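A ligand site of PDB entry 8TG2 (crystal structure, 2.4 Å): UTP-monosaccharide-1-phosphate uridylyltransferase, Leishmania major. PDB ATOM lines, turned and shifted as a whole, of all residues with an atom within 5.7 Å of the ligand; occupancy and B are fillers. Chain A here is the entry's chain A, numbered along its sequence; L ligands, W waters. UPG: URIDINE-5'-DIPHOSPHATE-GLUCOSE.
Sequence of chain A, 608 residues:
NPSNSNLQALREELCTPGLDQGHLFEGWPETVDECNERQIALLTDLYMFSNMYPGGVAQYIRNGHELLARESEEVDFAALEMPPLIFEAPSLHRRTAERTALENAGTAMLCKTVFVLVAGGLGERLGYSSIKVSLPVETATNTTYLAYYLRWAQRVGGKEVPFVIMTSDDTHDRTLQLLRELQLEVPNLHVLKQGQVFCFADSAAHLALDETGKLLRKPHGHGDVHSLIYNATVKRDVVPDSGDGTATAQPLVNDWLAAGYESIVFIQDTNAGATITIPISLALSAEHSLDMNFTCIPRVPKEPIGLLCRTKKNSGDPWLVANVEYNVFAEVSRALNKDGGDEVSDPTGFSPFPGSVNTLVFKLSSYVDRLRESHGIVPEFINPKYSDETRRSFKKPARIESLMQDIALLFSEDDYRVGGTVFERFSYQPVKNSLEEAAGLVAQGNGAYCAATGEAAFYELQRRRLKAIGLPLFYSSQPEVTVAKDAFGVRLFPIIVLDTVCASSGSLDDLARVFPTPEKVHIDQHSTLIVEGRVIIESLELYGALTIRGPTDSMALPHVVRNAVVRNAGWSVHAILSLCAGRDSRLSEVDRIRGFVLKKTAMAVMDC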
ATOM      1  N   LEU A 117     -10.147  25.392   9.223  1.00  0.00           N
ATOM      2  CA  LEU A 117     -11.019  24.351   9.834  1.00  0.00           C
ATOM      3  C   LEU A 117     -10.466  24.038  11.235  1.00  0.00           C
ATOM      4  O   LEU A 117      -9.302  23.622  11.358  1.00  0.00           O
ATOM      5  CB  LEU A 117     -11.052  23.111   8.944  1.00  0.00           C
ATOM      6  CG  LEU A 117     -11.632  21.843   9.600  1.00  0.00           C
ATOM      7  CD1 LEU A 117     -13.077  22.050  10.025  1.00  0.00           C
ATOM      8  CD2 LEU A 117     -11.554  20.681   8.629  1.00  0.00           C
ATOM      9  N   VAL A 118     -11.314  24.217  12.232  1.00  0.00           N
ATOM     10  CA  VAL A 118     -10.952  23.864  13.635  1.00  0.00           C
ATOM     11  C   VAL A 118     -11.370  22.411  13.880  1.00  0.00           C
ATOM     12  O   VAL A 118     -12.571  22.151  13.901  1.00  0.00           O
ATOM     13  CB  VAL A 118     -11.584  24.848  14.643  1.00  0.00           C
ATOM     14  CG1 VAL A 118     -10.846  26.192  14.587  1.00  0.00           C
ATOM     15  CG2 VAL A 118     -13.067  25.092  14.409  1.00  0.00           C
ATOM     16  N   ALA A 119     -10.376  21.538  14.012  1.00  0.00           N
ATOM     17  CA  ALA A 119     -10.580  20.076  14.171  1.00  0.00           C
ATOM     18  C   ALA A 119      -9.630  19.562  15.243  1.00  0.00           C
ATOM     19  O   ALA A 119      -8.965  18.566  15.056  1.00  0.00           O
ATOM     20  CB  ALA A 119     -10.391  19.379  12.855  1.00  0.00           C
ATOM     21  N   GLY A 120      -9.637  20.234  16.394  1.00  0.00           N
ATOM     22  CA  GLY A 120      -8.835  19.800  17.558  1.00  0.00           C
ATOM     23  C   GLY A 120      -9.669  19.063  18.582  1.00  0.00           C
ATOM     24  O   GLY A 120      -9.078  18.507  19.503  1.00  0.00           O
ATOM     25  N   GLY A 121     -10.992  19.010  18.405  1.00  0.00           N
ATOM     26  CA  GLY A 121     -11.904  18.524  19.440  1.00  0.00           C
ATOM     27  C   GLY A 121     -12.157  17.043  19.352  1.00  0.00           C
ATOM     28  O   GLY A 121     -12.166  16.515  18.229  1.00  0.00           O
ATOM     29  N   LEU A 122     -12.388  16.413  20.510  1.00  0.00           N
ATOM     30  CA  LEU A 122     -12.802  14.988  20.594  1.00  0.00           C
ATOM     31  C   LEU A 122     -14.305  14.854  20.345  1.00  0.00           C
ATOM     32  O   LEU A 122     -15.062  15.809  20.642  1.00  0.00           O
ATOM     33  CB  LEU A 122     -12.517  14.438  21.997  1.00  0.00           C
ATOM     34  CG  LEU A 122     -11.117  14.674  22.545  1.00  0.00           C
ATOM     35  CD1 LEU A 122     -11.152  14.772  24.066  1.00  0.00           C
ATOM     36  CD2 LEU A 122     -10.216  13.533  22.102  1.00  0.00           C
ATOM     37  N   LYS A 132     -13.539  13.496  14.604  1.00  0.00           N
ATOM     38  CA  LYS A 132     -14.856  13.926  14.107  1.00  0.00           C
ATOM     39  C   LYS A 132     -14.836  14.138  12.602  1.00  0.00           C
ATOM     40  O   LYS A 132     -15.861  13.854  11.966  1.00  0.00           O
ATOM     41  CB  LYS A 132     -15.295  15.184  14.853  1.00  0.00           C
ATOM     42  CG  LYS A 132     -15.608  14.904  16.310  1.00  0.00           C
ATOM     43  CD  LYS A 132     -16.289  16.028  17.018  1.00  0.00           C
ATOM     44  CE  LYS A 132     -17.776  16.076  16.755  1.00  0.00           C
ATOM     45  NZ  LYS A 132     -18.350  17.356  17.237  1.00  0.00           N
ATOM     46  N   MET A 166      -6.526  23.237  12.156  1.00  0.00           N
ATOM     47  CA  MET A 166      -6.039  23.170  13.546  1.00  0.00           C
ATOM     48  C   MET A 166      -6.308  21.772  14.099  1.00  0.00           C
ATOM     49  O   MET A 166      -7.443  21.297  14.042  1.00  0.00           O
ATOM     50  CB  MET A 166      -6.700  24.195  14.450  1.00  0.00           C
ATOM     51  CG  MET A 166      -6.123  24.122  15.839  1.00  0.00           C
ATOM     52  SD  MET A 166      -6.360  25.612  16.783  1.00  0.00           S
ATOM     53  CE  MET A 166      -8.108  25.474  17.148  1.00  0.00           C
ATOM     54  N   GLN A 194      -2.361  22.580  18.068  1.00  0.00           N
ATOM     55  CA  GLN A 194      -2.497  23.385  19.291  1.00  0.00           C
ATOM     56  C   GLN A 194      -1.962  22.593  20.471  1.00  0.00           C
ATOM     57  O   GLN A 194      -2.136  21.363  20.526  1.00  0.00           O
ATOM     58  CB  GLN A 194      -3.956  23.803  19.516  1.00  0.00           C
ATOM     59  CG  GLN A 194      -4.868  22.663  19.956  1.00  0.00           C
ATOM     60  CD  GLN A 194      -6.313  23.090  19.928  1.00  0.00           C
ATOM     61  OE1 GLN A 194      -7.113  22.567  19.153  1.00  0.00           O
ATOM     62  NE2 GLN A 194      -6.662  24.062  20.751  1.00  0.00           N
ATOM     63  N   PRO A 219      -7.321  20.748  26.716  1.00  0.00           N
ATOM     64  CA  PRO A 219      -7.363  21.682  25.605  1.00  0.00           C
ATOM     65  C   PRO A 219      -7.616  23.124  26.075  1.00  0.00           C
ATOM     66  O   PRO A 219      -8.352  23.336  27.010  1.00  0.00           O
ATOM     67  CB  PRO A 219      -8.558  21.214  24.759  1.00  0.00           C
ATOM     68  CG  PRO A 219      -8.753  19.764  25.169  1.00  0.00           C
ATOM     69  CD  PRO A 219      -8.378  19.717  26.634  1.00  0.00           C
ATOM     70  N   HIS A 220      -7.005  24.062  25.349  1.00  0.00           N
ATOM     71  CA  HIS A 220      -7.144  25.520  25.605  1.00  0.00           C
ATOM     72  C   HIS A 220      -8.307  26.102  24.794  1.00  0.00           C
ATOM     73  O   HIS A 220      -8.538  27.316  24.898  1.00  0.00           O
ATOM     74  CB  HIS A 220      -5.827  26.213  25.257  1.00  0.00           C
ATOM     75  CG  HIS A 220      -5.794  27.627  25.712  1.00  0.00           C
ATOM     76  ND1 HIS A 220      -5.756  28.682  24.838  1.00  0.00           N
ATOM     77  CD2 HIS A 220      -5.829  28.158  26.950  1.00  0.00           C
ATOM     78  CE1 HIS A 220      -5.738  29.814  25.534  1.00  0.00           C
ATOM     79  NE2 HIS A 220      -5.784  29.514  26.826  1.00  0.00           N
ATOM     80  N   GLY A 221      -8.990  25.306  23.982  1.00  0.00           N
ATOM     81  CA  GLY A 221     -10.153  25.797  23.207  1.00  0.00           C
ATOM     82  C   GLY A 221      -9.788  26.162  21.768  1.00  0.00           C
ATOM     83  O   GLY A 221      -8.602  26.231  21.407  1.00  0.00           O
ATOM     84  N   HIS A 222     -10.801  26.413  20.984  1.00  0.00           N
ATOM     85  CA  HIS A 222     -10.636  26.682  19.535  1.00  0.00           C
ATOM     86  C   HIS A 222     -10.167  28.123  19.303  1.00  0.00           C
ATOM     87  O   HIS A 222      -9.949  28.462  18.153  1.00  0.00           O
ATOM     88  CB  HIS A 222     -11.926  26.349  18.787  1.00  0.00           C
ATOM     89  CG  HIS A 222     -13.173  26.874  19.405  1.00  0.00           C
ATOM     90  ND1 HIS A 222     -13.515  28.207  19.377  1.00  0.00           N
ATOM     91  CD2 HIS A 222     -14.191  26.232  20.002  1.00  0.00           C
ATOM     92  CE1 HIS A 222     -14.686  28.376  19.949  1.00  0.00           C
ATOM     93  NE2 HIS A 222     -15.137  27.178  20.341  1.00  0.00           N
ATOM     94  N   ASP A 224      -7.299  29.099  19.911  1.00  0.00           N
ATOM     95  CA  ASP A 224      -5.840  28.917  19.637  1.00  0.00           C
ATOM     96  C   ASP A 224      -5.478  29.132  18.161  1.00  0.00           C
ATOM     97  O   ASP A 224      -4.271  29.253  17.911  1.00  0.00           O
ATOM     98  CB  ASP A 224      -5.410  27.528  20.075  1.00  0.00           C
ATOM     99  CG  ASP A 224      -5.354  27.393  21.585  1.00  0.00           C
ATOM    100  OD1 ASP A 224      -5.519  28.437  22.258  1.00  0.00           O
ATOM    101  OD2 ASP A 224      -5.119  26.262  22.099  1.00  0.00           O
ATOM    102  N   ILE A 267     -14.381  27.583   9.883  1.00  0.00           N
ATOM    103  CA  ILE A 267     -15.472  26.589   9.948  1.00  0.00           C
ATOM    104  C   ILE A 267     -15.115  25.525  10.995  1.00  0.00           C
ATOM    105  O   ILE A 267     -13.931  25.352  11.299  1.00  0.00           O
ATOM    106  CB  ILE A 267     -15.694  25.916   8.583  1.00  0.00           C
ATOM    107  CG1 ILE A 267     -14.457  25.153   8.116  1.00  0.00           C
ATOM    108  CG2 ILE A 267     -16.164  26.919   7.556  1.00  0.00           C
ATOM    109  CD1 ILE A 267     -14.753  24.121   7.055  1.00  0.00           C
ATOM    110  N   GLN A 268     -16.124  24.795  11.405  1.00  0.00           N
ATOM    111  CA  GLN A 268     -16.020  23.754  12.434  1.00  0.00           C
ATOM    112  C   GLN A 268     -16.140  22.388  11.770  1.00  0.00           C
ATOM    113  O   GLN A 268     -16.427  22.294  10.570  1.00  0.00           O
ATOM    114  CB  GLN A 268     -17.076  23.976  13.529  1.00  0.00           C
ATOM    115  CG  GLN A 268     -16.934  25.348  14.220  1.00  0.00           C
ATOM    116  CD  GLN A 268     -17.644  25.489  15.552  1.00  0.00           C
ATOM    117  OE1 GLN A 268     -17.078  26.013  16.507  1.00  0.00           O
ATOM    118  NE2 GLN A 268     -18.860  24.977  15.624  1.00  0.00           N
ATOM    119  N   ASP A 269     -15.962  21.348  12.557  1.00  0.00           N
ATOM    120  CA  ASP A 269     -15.611  20.004  12.080  1.00  0.00           C
ATOM    121  C   ASP A 269     -16.812  19.280  11.475  1.00  0.00           C
ATOM    122  O   ASP A 269     -16.550  18.464  10.579  1.00  0.00           O
ATOM    123  CB  ASP A 269     -14.974  19.186  13.185  1.00  0.00           C
ATOM    124  CG  ASP A 269     -15.659  19.249  14.531  1.00  0.00           C
ATOM    125  OD1 ASP A 269     -16.766  19.810  14.629  1.00  0.00           O
ATOM    126  OD2 ASP A 269     -15.059  18.750  15.464  1.00  0.00           O
ATOM    127  N   THR A 270     -18.037  19.492  11.924  1.00  0.00           N
ATOM    128  CA  THR A 270     -19.129  18.590  11.499  1.00  0.00           C
ATOM    129  C   THR A 270     -20.373  19.310  11.037  1.00  0.00           C
ATOM    130  O   THR A 270     -21.436  18.799  11.322  1.00  0.00           O
ATOM    131  CB  THR A 270     -19.490  17.593  12.585  1.00  0.00           C
ATOM    132  OG1 THR A 270     -19.833  18.289  13.788  1.00  0.00           O
ATOM    133  CG2 THR A 270     -18.352  16.618  12.827  1.00  0.00           C
ATOM    134  N   PRO A 304     -28.105  25.065  22.900  1.00  0.00           N
ATOM    135  CA  PRO A 304     -26.687  25.135  23.217  1.00  0.00           C
ATOM    136  C   PRO A 304     -25.856  25.842  22.141  1.00  0.00           C
ATOM    137  O   PRO A 304     -24.825  25.334  21.732  1.00  0.00           O
ATOM    138  CB  PRO A 304     -26.261  23.663  23.369  1.00  0.00           C
ATOM    139  CG  PRO A 304     -27.548  22.875  23.367  1.00  0.00           C
ATOM    140  CD  PRO A 304     -28.532  23.698  22.565  1.00  0.00           C
ATOM    141  N   ILE A 305     -26.314  27.022  21.696  1.00  0.00           N
ATOM    142  CA  ILE A 305     -25.514  27.886  20.783  1.00  0.00           C
ATOM    143  C   ILE A 305     -25.549  29.320  21.297  1.00  0.00           C
ATOM    144  O   ILE A 305     -26.562  29.730  21.892  1.00  0.00           O
ATOM    145  CB  ILE A 305     -26.022  27.818  19.349  1.00  0.00           C
ATOM    146  CG1 ILE A 305     -27.401  28.447  19.221  1.00  0.00           C
ATOM    147  CG2 ILE A 305     -26.017  26.381  18.848  1.00  0.00           C
ATOM    148  CD1 ILE A 305     -27.771  28.818  17.821  1.00  0.00           C
ATOM    149  N   GLY A 306     -24.481  30.049  21.042  1.00  0.00           N
ATOM    150  CA  GLY A 306     -24.341  31.429  21.542  1.00  0.00           C
ATOM    151  C   GLY A 306     -25.220  32.402  20.796  1.00  0.00           C
ATOM    152  O   GLY A 306     -25.846  32.023  19.774  1.00  0.00           O
ATOM    153  N   ASN A 323     -20.180  37.653  20.564  1.00  0.00           N
ATOM    154  CA  ASN A 323     -20.989  36.451  20.868  1.00  0.00           C
ATOM    155  C   ASN A 323     -21.041  36.313  22.380  1.00  0.00           C
ATOM    156  O   ASN A 323     -19.972  36.451  23.025  1.00  0.00           O
ATOM    157  CB  ASN A 323     -20.406  35.207  20.186  1.00  0.00           C
ATOM    158  CG  ASN A 323     -20.970  33.924  20.729  1.00  0.00           C
ATOM    159  OD1 ASN A 323     -22.122  33.584  20.438  1.00  0.00           O
ATOM    160  ND2 ASN A 323     -20.187  33.201  21.509  1.00  0.00           N
ATOM    161  N   GLU A 325     -22.012  33.316  24.980  1.00  0.00           N
ATOM    162  CA  GLU A 325     -22.272  31.861  25.044  1.00  0.00           C
ATOM    163  C   GLU A 325     -23.565  31.577  25.792  1.00  0.00           C
ATOM    164  O   GLU A 325     -24.046  32.432  26.544  1.00  0.00           O
ATOM    165  CB  GLU A 325     -21.105  31.110  25.696  1.00  0.00           C
ATOM    166  CG  GLU A 325     -19.954  30.828  24.748  1.00  0.00           C
ATOM    167  CD  GLU A 325     -20.262  29.900  23.583  1.00  0.00           C
ATOM    168  OE1 GLU A 325     -19.648  28.818  23.499  1.00  0.00           O
ATOM    169  OE2 GLU A 325     -21.110  30.261  22.744  1.00  0.00           O
ATOM    170  N   TYR A 326     -24.114  30.386  25.570  1.00  0.00           N
ATOM    171  CA  TYR A 326     -25.492  30.021  25.991  1.00  0.00           C
ATOM    172  C   TYR A 326     -25.619  30.155  27.515  1.00  0.00           C
ATOM    173  O   TYR A 326     -26.613  30.763  27.965  1.00  0.00           O
ATOM    174  CB  TYR A 326     -25.853  28.621  25.506  1.00  0.00           C
ATOM    175  CG  TYR A 326     -24.712  27.629  25.484  1.00  0.00           C
ATOM    176  CD1 TYR A 326     -23.873  27.522  24.380  1.00  0.00           C
ATOM    177  CD2 TYR A 326     -24.462  26.788  26.565  1.00  0.00           C
ATOM    178  CE1 TYR A 326     -22.820  26.625  24.343  1.00  0.00           C
ATOM    179  CE2 TYR A 326     -23.413  25.878  26.538  1.00  0.00           C
ATOM    180  CZ  TYR A 326     -22.592  25.785  25.427  1.00  0.00           C
ATOM    181  OH  TYR A 326     -21.551  24.886  25.371  1.00  0.00           O
ATOM    182  N   SER A 356     -25.444  32.388  16.940  1.00  0.00           N
ATOM    183  CA  SER A 356     -24.181  32.290  16.169  1.00  0.00           C
ATOM    184  C   SER A 356     -23.856  30.812  15.940  1.00  0.00           C
ATOM    185  O   SER A 356     -23.813  30.014  16.896  1.00  0.00           O
ATOM    186  CB  SER A 356     -23.056  32.959  16.881  1.00  0.00           C
ATOM    187  OG  SER A 356     -21.844  32.744  16.181  1.00  0.00           O
ATOM    188  N   VAL A 357     -23.592  30.481  14.683  1.00  0.00           N
ATOM    189  CA  VAL A 357     -23.291  29.088  14.260  1.00  0.00           C
ATOM    190  C   VAL A 357     -21.779  28.885  14.311  1.00  0.00           C
ATOM    191  O   VAL A 357     -21.356  27.733  14.308  1.00  0.00           O
ATOM    192  CB  VAL A 357     -23.906  28.894  12.853  1.00  0.00           C
ATOM    193  CG1 VAL A 357     -23.146  27.907  12.000  1.00  0.00           C
ATOM    194  CG2 VAL A 357     -25.365  28.522  12.981  1.00  0.00           C
ATOM    195  N   ASN A 358     -20.978  29.947  14.395  1.00  0.00           N
ATOM    196  CA  ASN A 358     -19.483  29.879  14.444  1.00  0.00           C
ATOM    197  C   ASN A 358     -18.913  29.428  13.084  1.00  0.00           C
ATOM    198  O   ASN A 358     -17.884  28.708  13.038  1.00  0.00           O
ATOM    199  CB  ASN A 358     -18.991  28.975  15.573  1.00  0.00           C
ATOM    200  CG  ASN A 358     -17.955  29.633  16.447  1.00  0.00           C
ATOM    201  OD1 ASN A 358     -17.842  30.849  16.490  1.00  0.00           O
ATOM    202  ND2 ASN A 358     -17.195  28.852  17.177  1.00  0.00           N
ATOM    203  N   ARG A 399      -9.233  24.153  33.506  1.00  0.00           N
ATOM    204  CA  ARG A 399      -8.216  24.697  32.572  1.00  0.00           C
ATOM    205  C   ARG A 399      -8.710  26.044  32.058  1.00  0.00           C
ATOM    206  O   ARG A 399      -9.945  26.237  31.994  1.00  0.00           O
ATOM    207  CB  ARG A 399      -8.019  23.739  31.385  1.00  0.00           C
ATOM    208  CG  ARG A 399      -9.222  23.715  30.449  1.00  0.00           C
ATOM    209  CD  ARG A 399      -9.492  22.340  29.884  1.00  0.00           C
ATOM    210  NE  ARG A 399     -10.890  22.065  29.625  1.00  0.00           N
ATOM    211  CZ  ARG A 399     -11.435  22.057  28.420  1.00  0.00           C
ATOM    212  NH1 ARG A 399     -10.703  22.348  27.358  1.00  0.00           N
ATOM    213  NH2 ARG A 399     -12.720  21.777  28.269  1.00  0.00           N
ATOM    214  N   LEU A 403     -12.251  31.177  23.012  1.00  0.00           N
ATOM    215  CA  LEU A 403     -13.179  30.984  21.885  1.00  0.00           C
ATOM    216  C   LEU A 403     -12.627  31.777  20.706  1.00  0.00           C
ATOM    217  O   LEU A 403     -12.201  32.917  20.899  1.00  0.00           O
ATOM    218  CB  LEU A 403     -14.581  31.478  22.247  1.00  0.00           C
ATOM    219  CG  LEU A 403     -15.211  30.874  23.495  1.00  0.00           C
ATOM    220  CD1 LEU A 403     -16.497  31.619  23.825  1.00  0.00           C
ATOM    221  CD2 LEU A 403     -15.497  29.399  23.320  1.00  0.00           C
ATOM    222  N   GLN A 405     -14.306  32.970  18.200  1.00  0.00           N
ATOM    223  CA  GLN A 405     -15.209  34.089  17.866  1.00  0.00           C
ATOM    224  C   GLN A 405     -14.900  35.320  18.733  1.00  0.00           C
ATOM    225  O   GLN A 405     -15.230  36.443  18.321  1.00  0.00           O
ATOM    226  CB  GLN A 405     -16.670  33.702  18.024  1.00  0.00           C
ATOM    227  CG  GLN A 405     -17.018  33.216  19.424  1.00  0.00           C
ATOM    228  CD  GLN A 405     -16.958  31.721  19.540  1.00  0.00           C
ATOM    229  OE1 GLN A 405     -15.950  31.107  19.209  1.00  0.00           O
ATOM    230  NE2 GLN A 405     -18.035  31.147  20.066  1.00  0.00           N
ATOM    231  N   TYR A 428     -28.038  24.925   9.385  1.00  0.00           N
ATOM    232  CA  TYR A 428     -27.145  24.525  10.499  1.00  0.00           C
ATOM    233  C   TYR A 428     -27.386  23.048  10.762  1.00  0.00           C
ATOM    234  O   TYR A 428     -28.475  22.691  11.259  1.00  0.00           O
ATOM    235  CB  TYR A 428     -27.433  25.397  11.713  1.00  0.00           C
ATOM    236  CG  TYR A 428     -26.613  25.085  12.931  1.00  0.00           C
ATOM    237  CD1 TYR A 428     -25.242  25.127  12.879  1.00  0.00           C
ATOM    238  CD2 TYR A 428     -27.219  24.791  14.140  1.00  0.00           C
ATOM    239  CE1 TYR A 428     -24.471  24.880  14.005  1.00  0.00           C
ATOM    240  CE2 TYR A 428     -26.466  24.536  15.268  1.00  0.00           C
ATOM    241  CZ  TYR A 428     -25.091  24.591  15.206  1.00  0.00           C
ATOM    242  OH  TYR A 428     -24.374  24.289  16.316  1.00  0.00           O
ATOM    243  N   PRO A 430     -25.125  20.413  12.465  1.00  0.00           N
ATOM    244  CA  PRO A 430     -23.999  19.785  13.138  1.00  0.00           C
ATOM    245  C   PRO A 430     -24.319  18.369  13.655  1.00  0.00           C
ATOM    246  O   PRO A 430     -25.472  18.022  13.879  1.00  0.00           O
ATOM    247  CB  PRO A 430     -23.756  20.738  14.312  1.00  0.00           C
ATOM    248  CG  PRO A 430     -25.140  21.210  14.652  1.00  0.00           C
ATOM    249  CD  PRO A 430     -25.827  21.371  13.320  1.00  0.00           C
ATOM    250  N   LYS A 432     -23.390  16.764  16.938  1.00  0.00           N
ATOM    251  CA  LYS A 432     -22.819  17.088  18.275  1.00  0.00           C
ATOM    252  C   LYS A 432     -23.243  16.078  19.328  1.00  0.00           C
ATOM    253  O   LYS A 432     -22.466  15.897  20.255  1.00  0.00           O
ATOM    254  CB  LYS A 432     -23.254  18.503  18.665  1.00  0.00           C
ATOM    255  CG  LYS A 432     -22.566  19.600  17.887  1.00  0.00           C
ATOM    256  CD  LYS A 432     -22.210  20.798  18.737  1.00  0.00           C
ATOM    257  CE  LYS A 432     -21.323  21.780  18.011  1.00  0.00           C
ATOM    258  NZ  LYS A 432     -20.684  22.730  18.956  1.00  0.00           N
HETATM  259  N1  UPG L   1     -12.214  22.743  18.796  1.00  0.00           N
HETATM  260  C2  UPG L   1     -10.847  22.725  18.550  1.00  0.00           C
HETATM  261  N3  UPG L   1     -10.050  22.787  19.657  1.00  0.00           N
HETATM  262  C4  UPG L   1     -10.470  22.868  20.982  1.00  0.00           C
HETATM  263  C5  UPG L   1     -11.893  22.869  21.153  1.00  0.00           C
HETATM  264  C6  UPG L   1     -12.698  22.811  20.087  1.00  0.00           C
HETATM  265  O2  UPG L   1     -10.388  22.675  17.414  1.00  0.00           O
HETATM  266  O4  UPG L   1      -9.641  22.910  21.882  1.00  0.00           O
HETATM  267  C1C UPG L   1     -13.110  22.720  17.642  1.00  0.00           C
HETATM  268  C2C UPG L   1     -13.921  21.427  17.528  1.00  0.00           C
HETATM  269  O2C UPG L   1     -13.149  20.420  16.925  1.00  0.00           O
HETATM  270  C3C UPG L   1     -15.087  21.904  16.652  1.00  0.00           C
HETATM  271  C4C UPG L   1     -15.281  23.362  17.116  1.00  0.00           C
HETATM  272  O4C UPG L   1     -14.061  23.736  17.803  1.00  0.00           O
HETATM  273  O3C UPG L   1     -14.776  21.881  15.262  1.00  0.00           O
HETATM  274  C5C UPG L   1     -16.443  23.633  18.024  1.00  0.00           C
HETATM  275  O5C UPG L   1     -16.352  22.832  19.226  1.00  0.00           O
HETATM  276  PA  UPG L   1     -17.733  22.232  19.788  1.00  0.00           P
HETATM  277  O1A UPG L   1     -17.461  21.535  21.064  1.00  0.00           O
HETATM  278  O2A UPG L   1     -18.459  21.475  18.721  1.00  0.00           O
HETATM  279  O3A UPG L   1     -18.548  23.598  20.000  1.00  0.00           O
HETATM  280  PB  UPG L   1     -18.517  24.702  21.146  1.00  0.00           P
HETATM  281  O1B UPG L   1     -17.151  25.247  21.300  1.00  0.00           O
HETATM  282  O2B UPG L   1     -19.172  24.039  22.323  1.00  0.00           O
HETATM  283  O3B UPG L   1     -19.440  25.843  20.493  1.00  0.00           O
HETATM  284  C1' UPG L   1     -19.054  26.550  19.360  1.00  0.00           C
HETATM  285  C2' UPG L   1     -19.119  28.048  19.639  1.00  0.00           C
HETATM  286  C3' UPG L   1     -20.552  28.501  19.842  1.00  0.00           C
HETATM  287  C4' UPG L   1     -21.395  28.054  18.663  1.00  0.00           C
HETATM  288  C5' UPG L   1     -21.275  26.550  18.458  1.00  0.00           C
HETATM  289  C6' UPG L   1     -21.985  26.083  17.190  1.00  0.00           C
HETATM  290  O2' UPG L   1     -18.361  28.352  20.782  1.00  0.00           O
HETATM  291  O3' UPG L   1     -20.609  29.919  19.965  1.00  0.00           O
HETATM  292  O4' UPG L   1     -22.759  28.382  18.882  1.00  0.00           O
HETATM  293  O5' UPG L   1     -19.909  26.185  18.297  1.00  0.00           O
HETATM  294  O6' UPG L   1     -21.935  24.674  17.039  1.00  0.00           O
HETATM  295  O   HOH W   1     -12.405  17.669  15.569  1.00  0.00           O
HETATM  296  O   HOH W   2     -20.810  23.475  14.277  1.00  0.00           O
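NZ of Lys 432 is in salt-bridge range of O2A of the ligand, 2.6 Å away. O6' of the ligand is in hydrogen-bond range of OH of Tyr 428. The backbone carbonyl oxygen (O) of Val 118 is in hydrogen-bond range of an oxygen (O3C) of the ligand. The backbone NH (N) of Gly 120 sits at hydrogen-bond distance from an oxygen (O2) of the ligand (2.8 Å). An oxygen (O4') of the ligand lies within hydrogen-bond range of the backbone carbonyl oxygen (O) of Ser 356, at 2.8 Å. An oxygen (O3') of the ligand lies within hydrogen-bond range of the side-chain carboxylate (OE2) of Glu 325 (2.8 Å). The side-chain amide nitrogen of Gln 405 sits at hydrogen-bond distance from an oxygen (O3') of the ligand, 2.9 Å away. O3C of the ligand lies close to N of Asp 269, at 3.0 Å. The side-chain carboxylate (OD2) of Asp 269 lies within hydrogen-bond range of an oxygen (O2C) of the ligand. The side-chain amide nitrogen (NE2) of Gln 268 sits at hydrogen-bond distance from an oxygen (O5') of the ligand (3.1 Å). A ring nitrogen (NE2) of His 222 lies within hydrogen-bond range of an oxygen (O1B) of the ligand (3.0 Å). An oxygen (O2C) of the ligand is in hydrogen-bond range of the backbone NH of Gly 121, 3.0 Å away. N3 of the ligand lies within hydrogen-bond range of OE1 of Gln 194. An oxygen (O4) of the ligand sits close to the backbone NH (N) of Gly 221, 3.3 Å away. The backbone NH (N) of Gly 306 is in hydrogen-bond range of an oxygen (O4') of the ligand (3.2 Å).
N of Val 118 lies within hydrogen-bond range of O of Ile 267, at 3.0 Å. O of Gly 306 lies within hydrogen-bond range of N of Ser 356 (2.9 Å). The backbone NH (N) of Asn 358 lies close to the side-chain hydroxyl (OG) of Ser 356 (3.4 Å). OE1 of Gln 405 sits at hydrogen-bond distance from ND2 of Asn 358. The side-chain amide nitrogen (ND2) of Asn 323 sits close to the side-chain amide nitrogen (NE2) of Gln 405. NE2 of Gln 194 sits at hydrogen-bond distance from O of Gly 221 (3.0 Å). The side-chain amide nitrogen (NE2) of Gln 194 sits at hydrogen-bond distance from the side-chain carboxylate (OD2) of Asp 224 (3.0 Å). The backbone NH of Ala 119 is in hydrogen-bond range of the backbone carbonyl oxygen of Met 166 (2.9 Å).
Ala 119 touches the ligand. CE of Met 166 touches O2 of the ligand (3.6 Å). CB of Pro 219 touches O4 of the ligand, 3.5 Å away. Ile 305 touches the ligand. ND2 of Asn 323 touches O3' of the ligand, at 3.7 Å. Tyr 326 touches the ligand (OH to O2B, 3.96 Å). O of Val 357 touches C6' of the ligand, 3.4 Å away. ND2 of Asn 358 touches C2' of the ligand, 3.2 Å away. Leu 403 touches the ligand (CD2 to O2', 3.97 Å). Of the 33 residues printed, 23 come within 4 Å of the ligand. The nearest printed residue that does not touch the ligand is Lys 132 (4.4 Å).
Water W1 lies within hydrogen-bond range of the side-chain carboxylate of Asp 269 (2.9 Å), the backbone carbonyl oxygen of Gly 121 (2.9 Å) and an oxygen (O2C) of the ligand (3.2 Å). Water W2 bridges NE2 of Gln 268 and O6' of the ligand.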
